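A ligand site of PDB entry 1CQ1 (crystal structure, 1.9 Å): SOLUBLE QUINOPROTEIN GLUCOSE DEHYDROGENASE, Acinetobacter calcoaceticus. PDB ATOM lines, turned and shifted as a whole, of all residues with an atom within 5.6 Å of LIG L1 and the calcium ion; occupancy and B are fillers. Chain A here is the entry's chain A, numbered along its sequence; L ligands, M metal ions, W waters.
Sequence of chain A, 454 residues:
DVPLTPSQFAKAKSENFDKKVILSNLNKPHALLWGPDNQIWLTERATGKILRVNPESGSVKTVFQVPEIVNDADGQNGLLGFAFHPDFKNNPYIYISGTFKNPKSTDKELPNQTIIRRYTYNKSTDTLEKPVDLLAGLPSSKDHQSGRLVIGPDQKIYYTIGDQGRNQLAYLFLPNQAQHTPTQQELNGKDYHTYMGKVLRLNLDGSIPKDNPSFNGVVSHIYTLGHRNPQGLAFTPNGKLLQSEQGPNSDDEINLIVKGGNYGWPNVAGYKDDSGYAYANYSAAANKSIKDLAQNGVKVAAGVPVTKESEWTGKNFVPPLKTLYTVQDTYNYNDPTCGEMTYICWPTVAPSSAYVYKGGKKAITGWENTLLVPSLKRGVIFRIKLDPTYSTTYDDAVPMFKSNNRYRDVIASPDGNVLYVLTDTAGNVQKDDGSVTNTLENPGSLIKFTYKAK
N of Gly 247 is in hydrogen-bond range of OD1 of Asp 252 (2.7 Å).
The backbone NH of Leu 376 sits at hydrogen-bond distance from the backbone carbonyl oxygen of Ala 350, at 3.0 Å.
The backbone NH (N) of Gln 246 lies within hydrogen-bond range of the backbone carbonyl oxygen (O) of Asn 229, 3.0 Å away.
NZ of Lys 377 sits at hydrogen-bond distance from O of Tyr 343 (2.9 Å).
NH1 of Arg 228 is in hydrogen-bond range of O of Gln 246, 3.1 Å away.
O of Asn 428 lies within hydrogen-bond range of NH1 of Arg 406, at 3.0 Å.
NE of Arg 406 is in salt-bridge range of OD2 of Asp 424 (2.8 Å).
The side-chain carboxylate of Asp 143 lies within hydrogen-bond range of the side-chain amide nitrogen of Gln 76 (3.3 Å).
The backbone carbonyl oxygen of Tyr 343 lies close to an oxygen (O6) of LIG L1, 3.5 Å away.
NE2 of Gln 76 touches C3 of LIG L1, at 3.4 Å.
CE3 of Trp 346 touches O5 of LIG L1 (3.6 Å).
CB of Ala 350 touches C12 of LIG L1, at 3.7 Å.
Leu 376 touches LIG L1.
Hydrophobic or aromatic side chains that line LIG L1: His 144, Tyr 343, Trp 346, Ala 350 and Leu 376.
Along chain A the residues within 4 Å of LIG L1 span positions 76 to 408.
Of the 23 residues printed, 2 come within 4 Å of the calcium ion.
Along chain A the residues within 4 Å of the calcium ion span positions 247 to 248.
The nearest printed residue that does not touch the calcium ion is Arg 228 (4.05 Å).
The calcium ion is bound by an oxygen (O5) of LIG L1 (2.3 Å).
O of Gly 247 binds the calcium ion, at 2.4 Å.
The calcium ion is bound by water W3, at 2.4 Å.
An oxygen (O4) of LIG L1 binds the calcium ion (2.4 Å).
The calcium ion is bound by N2 of LIG L1 (2.4 Å).
O of Pro 248 binds the calcium ion (2.4 Å).
Water W2 binds the calcium ion (2.5 Å).
Water W3 lies within hydrogen-bond range of the side-chain carboxylate of Asp 252 (2.7 Å) and the side-chain amide nitrogen of Gln 246 (2.8 Å).
Water W2 bridges an oxygen (O5) of LG2 L2 and the guanidinium group (NH2) of Arg 228.
Water W4 lies within hydrogen-bond range of an oxygen (O2) of LIG L1 and the guanidinium group (NH1) of Arg 408.
An oxygen (O3) of LIG L1 lies within hydrogen-bond range of a ring nitrogen (NE2) of His 144, 3.3 Å away.
The side-chain amide nitrogen (NE2) of Gln 246 sits close to an oxygen (O4) of LIG L1 (3.4 Å).
NE2 of Gln 76 lies within hydrogen-bond range of O2 of LG2 L2.
The side-chain amino group (NZ) of Lys 377 is in salt-bridge range of an oxygen (O6) of LIG L1, 2.6 Å away.
NH1 of Arg 228 is in hydrogen-bond range of O3 of LIG L1, at 3.4 Å.
OD1 of Asp 143 is in hydrogen-bond range of O2 of LG2 L2.
The guanidinium group of Arg 406 lies within salt-bridge range of an oxygen (O7) of LIG L1, 2.8 Å away.
A ring nitrogen (NE2) of His 144 is in hydrogen-bond range of an oxygen (O1) of LG2 L2 (3.0 Å).
An oxygen (O6) of LIG L1 lies within hydrogen-bond range of the side-chain hydroxyl (OG1) of Thr 348, 3.1 Å away.
The side-chain amide nitrogen (NE2) of Gln 231 sits at hydrogen-bond distance from an oxygen (O2) of LIG L1, 3.1 Å away.
An oxygen (O1) of LIG L1 lies within salt-bridge range of the guanidinium group (NH2) of Arg 408 (2.8 Å).
The side-chain amide nitrogen (ND2) of Asn 229 sits at hydrogen-bond distance from an oxygen (O3) of LIG L1, 3.0 Å away.
The guanidinium group (NH2) of Arg 228 lies within hydrogen-bond range of an oxygen (O1) of LG2 L2 (2.8 Å).
An oxygen (O1) of LG2 L2 sits close to an oxygen (O4) of LIG L1, at 3.3 Å.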
ATOM      1  N   GLN A  76     -12.088   8.434 -12.880  1.00  0.00           N
ATOM      2  CA  GLN A  76     -12.408   8.156 -14.273  1.00  0.00           C
ATOM      3  C   GLN A  76     -13.224   6.877 -14.371  1.00  0.00           C
ATOM      4  O   GLN A  76     -13.337   6.260 -15.425  1.00  0.00           O
ATOM      5  CB  GLN A  76     -11.100   8.026 -15.080  1.00  0.00           C
ATOM      6  CG  GLN A  76     -10.315   9.333 -15.128  1.00  0.00           C
ATOM      7  CD  GLN A  76      -8.897   9.176 -15.653  1.00  0.00           C
ATOM      8  OE1 GLN A  76      -8.497   8.118 -16.131  1.00  0.00           O
ATOM      9  NE2 GLN A  76      -8.115  10.245 -15.545  1.00  0.00           N
ATOM     10  N   ASP A 143      -8.317   5.526 -11.876  1.00  0.00           N
ATOM     11  CA  ASP A 143      -7.506   6.110 -12.952  1.00  0.00           C
ATOM     12  C   ASP A 143      -7.262   5.122 -14.089  1.00  0.00           C
ATOM     13  O   ASP A 143      -7.222   3.904 -13.909  1.00  0.00           O
ATOM     14  CB  ASP A 143      -6.179   6.574 -12.343  1.00  0.00           C
ATOM     15  CG  ASP A 143      -5.405   7.587 -13.158  1.00  0.00           C
ATOM     16  OD1 ASP A 143      -6.005   8.365 -13.933  1.00  0.00           O
ATOM     17  OD2 ASP A 143      -4.159   7.643 -13.048  1.00  0.00           O
ATOM     18  N   HIS A 144      -7.062   5.697 -15.265  1.00  0.00           N
ATOM     19  CA  HIS A 144      -6.717   4.864 -16.436  1.00  0.00           C
ATOM     20  C   HIS A 144      -7.562   3.614 -16.551  1.00  0.00           C
ATOM     21  O   HIS A 144      -7.063   2.494 -16.476  1.00  0.00           O
ATOM     22  CB  HIS A 144      -5.242   4.457 -16.362  1.00  0.00           C
ATOM     23  CG  HIS A 144      -4.308   5.629 -16.414  1.00  0.00           C
ATOM     24  ND1 HIS A 144      -2.961   5.486 -16.173  1.00  0.00           N
ATOM     25  CD2 HIS A 144      -4.511   6.946 -16.672  1.00  0.00           C
ATOM     26  CE1 HIS A 144      -2.382   6.670 -16.281  1.00  0.00           C
ATOM     27  NE2 HIS A 144      -3.288   7.565 -16.585  1.00  0.00           N
ATOM     28  N   ARG A 228      -1.105   1.922 -21.747  1.00  0.00           N
ATOM     29  CA  ARG A 228      -1.273   2.821 -20.611  1.00  0.00           C
ATOM     30  C   ARG A 228      -2.767   3.152 -20.447  1.00  0.00           C
ATOM     31  O   ARG A 228      -3.432   2.416 -19.701  1.00  0.00           O
ATOM     32  CB  ARG A 228      -0.445   4.079 -20.779  1.00  0.00           C
ATOM     33  CG  ARG A 228      -0.446   4.983 -19.544  1.00  0.00           C
ATOM     34  CD  ARG A 228       0.484   6.153 -19.766  1.00  0.00           C
ATOM     35  NE  ARG A 228       0.524   7.160 -18.726  1.00  0.00           N
ATOM     36  CZ  ARG A 228      -0.392   8.123 -18.597  1.00  0.00           C
ATOM     37  NH1 ARG A 228      -1.402   8.175 -19.454  1.00  0.00           N
ATOM     38  NH2 ARG A 228      -0.281   9.024 -17.613  1.00  0.00           N
ATOM     39  N   ASN A 229      -3.276   4.119 -21.193  1.00  0.00           N
ATOM     40  CA  ASN A 229      -4.710   4.414 -21.145  1.00  0.00           C
ATOM     41  C   ASN A 229      -5.313   4.593 -22.525  1.00  0.00           C
ATOM     42  O   ASN A 229      -5.460   5.720 -22.994  1.00  0.00           O
ATOM     43  CB  ASN A 229      -4.958   5.688 -20.303  1.00  0.00           C
ATOM     44  CG  ASN A 229      -6.434   5.953 -20.050  1.00  0.00           C
ATOM     45  OD1 ASN A 229      -7.268   5.056 -20.208  1.00  0.00           O
ATOM     46  ND2 ASN A 229      -6.763   7.175 -19.657  1.00  0.00           N
ATOM     47  N   GLN A 231      -8.009   5.084 -24.749  1.00  0.00           N
ATOM     48  CA  GLN A 231      -9.420   5.460 -24.752  1.00  0.00           C
ATOM     49  C   GLN A 231     -10.037   5.452 -26.138  1.00  0.00           C
ATOM     50  O   GLN A 231     -11.239   5.651 -26.295  1.00  0.00           O
ATOM     51  CB  GLN A 231      -9.564   6.868 -24.134  1.00  0.00           C
ATOM     52  CG  GLN A 231      -9.366   6.835 -22.624  1.00  0.00           C
ATOM     53  CD  GLN A 231      -9.282   8.198 -21.979  1.00  0.00           C
ATOM     54  OE1 GLN A 231      -8.797   9.193 -22.540  1.00  0.00           O
ATOM     55  NE2 GLN A 231      -9.766   8.293 -20.741  1.00  0.00           N
ATOM     56  N   GLN A 246      -3.372   7.448 -24.316  1.00  0.00           N
ATOM     57  CA  GLN A 246      -2.765   8.493 -23.511  1.00  0.00           C
ATOM     58  C   GLN A 246      -1.389   8.069 -23.011  1.00  0.00           C
ATOM     59  O   GLN A 246      -1.323   7.022 -22.364  1.00  0.00           O
ATOM     60  CB  GLN A 246      -3.643   8.741 -22.255  1.00  0.00           C
ATOM     61  CG  GLN A 246      -5.079   9.108 -22.638  1.00  0.00           C
ATOM     62  CD  GLN A 246      -5.432  10.544 -22.396  1.00  0.00           C
ATOM     63  OE1 GLN A 246      -6.621  10.925 -22.382  1.00  0.00           O
ATOM     64  NE2 GLN A 246      -4.440  11.388 -22.187  1.00  0.00           N
ATOM     65  N   GLY A 247      -0.380   8.897 -23.263  1.00  0.00           N
ATOM     66  CA  GLY A 247       0.955   8.584 -22.702  1.00  0.00           C
ATOM     67  C   GLY A 247       1.113   9.445 -21.436  1.00  0.00           C
ATOM     68  O   GLY A 247       0.161  10.133 -21.055  1.00  0.00           O
ATOM     69  N   PRO A 248       2.264   9.401 -20.790  1.00  0.00           N
ATOM     70  CA  PRO A 248       2.517  10.157 -19.562  1.00  0.00           C
ATOM     71  C   PRO A 248       2.726  11.628 -19.813  1.00  0.00           C
ATOM     72  O   PRO A 248       1.776  12.291 -20.262  1.00  0.00           O
ATOM     73  CB  PRO A 248       3.721   9.444 -18.974  1.00  0.00           C
ATOM     74  CG  PRO A 248       4.473   8.973 -20.189  1.00  0.00           C
ATOM     75  CD  PRO A 248       3.411   8.559 -21.171  1.00  0.00           C
ATOM     76  N   ASN A 249       3.919  12.193 -19.604  1.00  0.00           N
ATOM     77  CA  ASN A 249       4.135  13.605 -19.896  1.00  0.00           C
ATOM     78  C   ASN A 249       4.415  13.784 -21.391  1.00  0.00           C
ATOM     79  O   ASN A 249       4.531  14.899 -21.904  1.00  0.00           O
ATOM     80  CB  ASN A 249       5.282  14.268 -19.154  1.00  0.00           C
ATOM     81  CG  ASN A 249       5.344  14.058 -17.670  1.00  0.00           C
ATOM     82  OD1 ASN A 249       4.646  13.222 -17.098  1.00  0.00           O
ATOM     83  ND2 ASN A 249       6.240  14.839 -17.050  1.00  0.00           N
ATOM     84  N   SER A 250       4.496  12.658 -22.097  1.00  0.00           N
ATOM     85  CA  SER A 250       4.741  12.730 -23.531  1.00  0.00           C
ATOM     86  C   SER A 250       4.153  11.513 -24.228  1.00  0.00           C
ATOM     87  O   SER A 250       3.725  10.564 -23.582  1.00  0.00           O
ATOM     88  CB  SER A 250       6.267  12.746 -23.795  1.00  0.00           C
ATOM     89  OG  SER A 250       6.813  11.505 -23.368  1.00  0.00           O
ATOM     90  N   ASP A 252       1.765  10.494 -26.498  1.00  0.00           N
ATOM     91  CA  ASP A 252       0.416   9.940 -26.669  1.00  0.00           C
ATOM     92  C   ASP A 252       0.558   9.195 -28.009  1.00  0.00           C
ATOM     93  O   ASP A 252       1.390   9.668 -28.812  1.00  0.00           O
ATOM     94  CB  ASP A 252      -0.665  10.982 -26.848  1.00  0.00           C
ATOM     95  CG  ASP A 252      -0.955  11.810 -25.593  1.00  0.00           C
ATOM     96  OD1 ASP A 252      -0.772  11.259 -24.497  1.00  0.00           O
ATOM     97  OD2 ASP A 252      -1.356  12.970 -25.775  1.00  0.00           O
ATOM     98  N   TYR A 343       1.198  20.419 -15.864  1.00  0.00           N
ATOM     99  CA  TYR A 343       0.908  19.317 -16.764  1.00  0.00           C
ATOM    100  C   TYR A 343       0.320  19.765 -18.094  1.00  0.00           C
ATOM    101  O   TYR A 343       0.692  19.222 -19.131  1.00  0.00           O
ATOM    102  CB  TYR A 343       0.046  18.250 -16.097  1.00  0.00           C
ATOM    103  CG  TYR A 343      -1.431  18.517 -15.956  1.00  0.00           C
ATOM    104  CD1 TYR A 343      -2.326  18.122 -16.954  1.00  0.00           C
ATOM    105  CD2 TYR A 343      -1.958  19.132 -14.827  1.00  0.00           C
ATOM    106  CE1 TYR A 343      -3.687  18.350 -16.829  1.00  0.00           C
ATOM    107  CE2 TYR A 343      -3.311  19.361 -14.691  1.00  0.00           C
ATOM    108  CZ  TYR A 343      -4.176  18.968 -15.700  1.00  0.00           C
ATOM    109  OH  TYR A 343      -5.522  19.194 -15.570  1.00  0.00           O
ATOM    110  N   ILE A 344      -0.613  20.707 -18.089  1.00  0.00           N
ATOM    111  CA  ILE A 344      -1.256  21.135 -19.328  1.00  0.00           C
ATOM    112  C   ILE A 344      -0.209  21.526 -20.385  1.00  0.00           C
ATOM    113  O   ILE A 344      -0.492  21.454 -21.582  1.00  0.00           O
ATOM    114  CB  ILE A 344      -2.226  22.304 -19.061  1.00  0.00           C
ATOM    115  CG1 ILE A 344      -3.431  21.806 -18.254  1.00  0.00           C
ATOM    116  CG2 ILE A 344      -2.672  22.990 -20.341  1.00  0.00           C
ATOM    117  CD1 ILE A 344      -4.423  20.951 -19.025  1.00  0.00           C
ATOM    118  N   TRP A 346       2.661  20.134 -20.747  1.00  0.00           N
ATOM    119  CA  TRP A 346       3.393  18.936 -21.174  1.00  0.00           C
ATOM    120  C   TRP A 346       3.101  18.666 -22.657  1.00  0.00           C
ATOM    121  O   TRP A 346       2.010  18.961 -23.161  1.00  0.00           O
ATOM    122  CB  TRP A 346       3.047  17.713 -20.342  1.00  0.00           C
ATOM    123  CG  TRP A 346       3.509  17.639 -18.917  1.00  0.00           C
ATOM    124  CD1 TRP A 346       4.482  18.378 -18.313  1.00  0.00           C
ATOM    125  CD2 TRP A 346       3.008  16.744 -17.906  1.00  0.00           C
ATOM    126  NE1 TRP A 346       4.616  18.006 -16.992  1.00  0.00           N
ATOM    127  CE2 TRP A 346       3.725  17.007 -16.720  1.00  0.00           C
ATOM    128  CE3 TRP A 346       2.018  15.753 -17.894  1.00  0.00           C
ATOM    129  CZ2 TRP A 346       3.499  16.313 -15.540  1.00  0.00           C
ATOM    130  CZ3 TRP A 346       1.796  15.066 -16.709  1.00  0.00           C
ATOM    131  CH2 TRP A 346       2.529  15.342 -15.560  1.00  0.00           C
ATOM    132  N   THR A 348       1.878  16.622 -24.757  1.00  0.00           N
ATOM    133  CA  THR A 348       0.866  15.637 -24.999  1.00  0.00           C
ATOM    134  C   THR A 348      -0.428  16.311 -25.468  1.00  0.00           C
ATOM    135  O   THR A 348      -0.534  17.539 -25.439  1.00  0.00           O
ATOM    136  CB  THR A 348       0.472  14.827 -23.733  1.00  0.00           C
ATOM    137  OG1 THR A 348       0.397  15.738 -22.628  1.00  0.00           O
ATOM    138  CG2 THR A 348       1.474  13.735 -23.450  1.00  0.00           C
ATOM    139  N   ALA A 350      -3.619  14.456 -24.895  1.00  0.00           N
ATOM    140  CA  ALA A 350      -4.663  13.741 -24.171  1.00  0.00           C
ATOM    141  C   ALA A 350      -5.842  13.334 -25.037  1.00  0.00           C
ATOM    142  O   ALA A 350      -6.933  13.923 -25.009  1.00  0.00           O
ATOM    143  CB  ALA A 350      -5.120  14.607 -22.977  1.00  0.00           C
ATOM    144  N   LEU A 376      -8.592  16.384 -25.072  1.00  0.00           N
ATOM    145  CA  LEU A 376      -9.122  16.954 -23.841  1.00  0.00           C
ATOM    146  C   LEU A 376      -8.372  18.220 -23.470  1.00  0.00           C
ATOM    147  O   LEU A 376      -8.959  19.308 -23.463  1.00  0.00           O
ATOM    148  CB  LEU A 376      -9.006  15.950 -22.696  1.00  0.00           C
ATOM    149  CG  LEU A 376      -9.833  14.672 -22.829  1.00  0.00           C
ATOM    150  CD1 LEU A 376      -9.459  13.643 -21.767  1.00  0.00           C
ATOM    151  CD2 LEU A 376     -11.324  14.977 -22.761  1.00  0.00           C
ATOM    152  N   LYS A 377      -7.068  18.104 -23.228  1.00  0.00           N
ATOM    153  CA  LYS A 377      -6.281  19.244 -22.775  1.00  0.00           C
ATOM    154  C   LYS A 377      -6.040  20.333 -23.806  1.00  0.00           C
ATOM    155  O   LYS A 377      -5.755  21.471 -23.383  1.00  0.00           O
ATOM    156  CB  LYS A 377      -4.962  18.775 -22.162  1.00  0.00           C
ATOM    157  CG  LYS A 377      -3.818  18.478 -23.114  1.00  0.00           C
ATOM    158  CD  LYS A 377      -2.612  17.919 -22.361  1.00  0.00           C
ATOM    159  CE  LYS A 377      -1.353  18.737 -22.622  1.00  0.00           C
ATOM    160  NZ  LYS A 377      -0.268  18.335 -21.687  1.00  0.00           N
ATOM    161  N   ARG A 406     -13.115  20.599 -23.290  1.00  0.00           N
ATOM    162  CA  ARG A 406     -12.425  19.328 -23.240  1.00  0.00           C
ATOM    163  C   ARG A 406     -13.230  18.359 -24.112  1.00  0.00           C
ATOM    164  O   ARG A 406     -14.315  17.918 -23.733  1.00  0.00           O
ATOM    165  CB  ARG A 406     -12.278  18.815 -21.811  1.00  0.00           C
ATOM    166  CG  ARG A 406     -11.392  19.668 -20.922  1.00  0.00           C
ATOM    167  CD  ARG A 406     -11.445  19.211 -19.480  1.00  0.00           C
ATOM    168  NE  ARG A 406     -11.203  17.799 -19.240  1.00  0.00           N
ATOM    169  CZ  ARG A 406     -10.016  17.230 -19.096  1.00  0.00           C
ATOM    170  NH1 ARG A 406      -8.910  17.974 -19.156  1.00  0.00           N
ATOM    171  NH2 ARG A 406      -9.940  15.936 -18.872  1.00  0.00           N
ATOM    172  N   ARG A 408     -14.416  15.106 -25.711  1.00  0.00           N
ATOM    173  CA  ARG A 408     -14.397  13.750 -25.164  1.00  0.00           C
ATOM    174  C   ARG A 408     -14.673  12.637 -26.150  1.00  0.00           C
ATOM    175  O   ARG A 408     -14.302  11.481 -25.922  1.00  0.00           O
ATOM    176  CB  ARG A 408     -15.450  13.701 -24.024  1.00  0.00           C
ATOM    177  CG  ARG A 408     -15.719  12.368 -23.383  1.00  0.00           C
ATOM    178  CD  ARG A 408     -14.612  11.745 -22.571  1.00  0.00           C
ATOM    179  NE  ARG A 408     -13.994  12.646 -21.604  1.00  0.00           N
ATOM    180  CZ  ARG A 408     -12.949  12.321 -20.866  1.00  0.00           C
ATOM    181  NH1 ARG A 408     -12.395  11.108 -20.984  1.00  0.00           N
ATOM    182  NH2 ARG A 408     -12.431  13.187 -19.998  1.00  0.00           N
ATOM    183  N   ASP A 424     -16.409  17.706 -21.901  1.00  0.00           N
ATOM    184  CA  ASP A 424     -16.454  17.338 -20.482  1.00  0.00           C
ATOM    185  C   ASP A 424     -17.271  18.381 -19.703  1.00  0.00           C
ATOM    186  O   ASP A 424     -17.435  19.494 -20.176  1.00  0.00           O
ATOM    187  CB  ASP A 424     -15.075  17.243 -19.844  1.00  0.00           C
ATOM    188  CG  ASP A 424     -14.332  15.948 -20.165  1.00  0.00           C
ATOM    189  OD1 ASP A 424     -14.928  15.087 -20.822  1.00  0.00           O
ATOM    190  OD2 ASP A 424     -13.168  15.834 -19.730  1.00  0.00           O
ATOM    191  N   ASN A 428      -9.553  21.141 -16.694  1.00  0.00           N
ATOM    192  CA  ASN A 428      -8.657  22.134 -17.229  1.00  0.00           C
ATOM    193  C   ASN A 428      -8.469  22.019 -18.734  1.00  0.00           C
ATOM    194  O   ASN A 428      -8.401  20.915 -19.286  1.00  0.00           O
ATOM    195  CB  ASN A 428      -7.271  21.992 -16.565  1.00  0.00           C
ATOM    196  CG  ASN A 428      -7.337  22.164 -15.065  1.00  0.00           C
ATOM    197  OD1 ASN A 428      -6.722  21.403 -14.310  1.00  0.00           O
ATOM    198  ND2 ASN A 428      -8.105  23.157 -14.635  1.00  0.00           N
HETATM  199  N1  LIG L   1      -7.583  12.815 -18.937  1.00  0.00           N
HETATM  200  C1  LIG L   1      -8.232  11.631 -18.841  1.00  0.00           C
HETATM  201  C2  LIG L   1      -9.618  11.625 -18.702  1.00  0.00           C
HETATM  202  O1  LIG L   1     -10.220  12.673 -18.411  1.00  0.00           O
HETATM  203  O2  LIG L   1     -10.312  10.635 -18.836  1.00  0.00           O
HETATM  204  C3  LIG L   1      -7.304  10.604 -18.876  1.00  0.00           C
HETATM  205  C4  LIG L   1      -6.076  11.152 -19.011  1.00  0.00           C
HETATM  206  C5  LIG L   1      -6.243  12.514 -19.047  1.00  0.00           C
HETATM  207  C6  LIG L   1      -4.808  10.579 -19.147  1.00  0.00           C
HETATM  208  O3  LIG L   1      -4.601   9.208 -19.138  1.00  0.00           O
HETATM  209  C7  LIG L   1      -3.710  11.374 -19.328  1.00  0.00           C
HETATM  210  O4  LIG L   1      -2.480  10.798 -19.465  1.00  0.00           O
HETATM  211  C8  LIG L   1      -3.851  12.783 -19.362  1.00  0.00           C
HETATM  212  N2  LIG L   1      -2.671  13.395 -19.573  1.00  0.00           N
HETATM  213  C9  LIG L   1      -2.701  14.712 -19.684  1.00  0.00           C
HETATM  214  C10 LIG L   1      -1.430  15.235 -20.002  1.00  0.00           C
HETATM  215  O5  LIG L   1      -0.455  14.464 -20.226  1.00  0.00           O
HETATM  216  O6  LIG L   1      -1.255  16.489 -20.076  1.00  0.00           O
HETATM  217  C11 LIG L   1      -3.885  15.399 -19.539  1.00  0.00           C
HETATM  218  C12 LIG L   1      -5.111  14.756 -19.292  1.00  0.00           C
HETATM  219  C13 LIG L   1      -6.300  15.522 -19.074  1.00  0.00           C
HETATM  220  O7  LIG L   1      -6.512  16.606 -19.623  1.00  0.00           O
HETATM  221  O8  LIG L   1      -7.200  15.165 -18.322  1.00  0.00           O
HETATM  222  C14 LIG L   1      -5.133  13.374 -19.217  1.00  0.00           C
HETATM  223  C1  LG2 L   2      -4.221  11.379 -15.084  1.00  0.00           C
HETATM  224  C2  LG2 L   2      -5.004  12.695 -14.997  1.00  0.00           C
HETATM  225  C3  LG2 L   2      -3.967  13.750 -14.633  1.00  0.00           C
HETATM  226  C4  LG2 L   2      -2.930  13.898 -15.762  1.00  0.00           C
HETATM  227  C5  LG2 L   2      -1.691  14.709 -15.411  1.00  0.00           C
HETATM  228  C6  LG2 L   2      -3.126  11.539 -16.186  1.00  0.00           C
HETATM  229  O1  LG2 L   2      -2.300  10.357 -16.187  1.00  0.00           O
HETATM  230  O2  LG2 L   2      -5.177  10.326 -15.383  1.00  0.00           O
HETATM  231  O3  LG2 L   2      -5.857  12.647 -13.833  1.00  0.00           O
HETATM  232  O4  LG2 L   2      -4.564  15.005 -14.557  1.00  0.00           O
HETATM  233  O5  LG2 L   2      -2.208  12.616 -15.862  1.00  0.00           O
HETATM  234  O6  LG2 L   2      -1.037  14.334 -14.230  1.00  0.00           O
HETATM  235 CA    CA M   1      -0.657  12.156 -20.148  1.00  0.00          CA
HETATM  236  O   HOH W   1     -12.036  12.880 -16.287  1.00  0.00           O
HETATM  237  O   HOH W   2      -0.142  12.207 -17.743  1.00  0.00           O
HETATM  238  O   HOH W   3      -1.810  12.239 -22.216  1.00  0.00           O
HETATM  239  O   HOH W   4     -12.932  10.210 -17.835  1.00  0.00           O
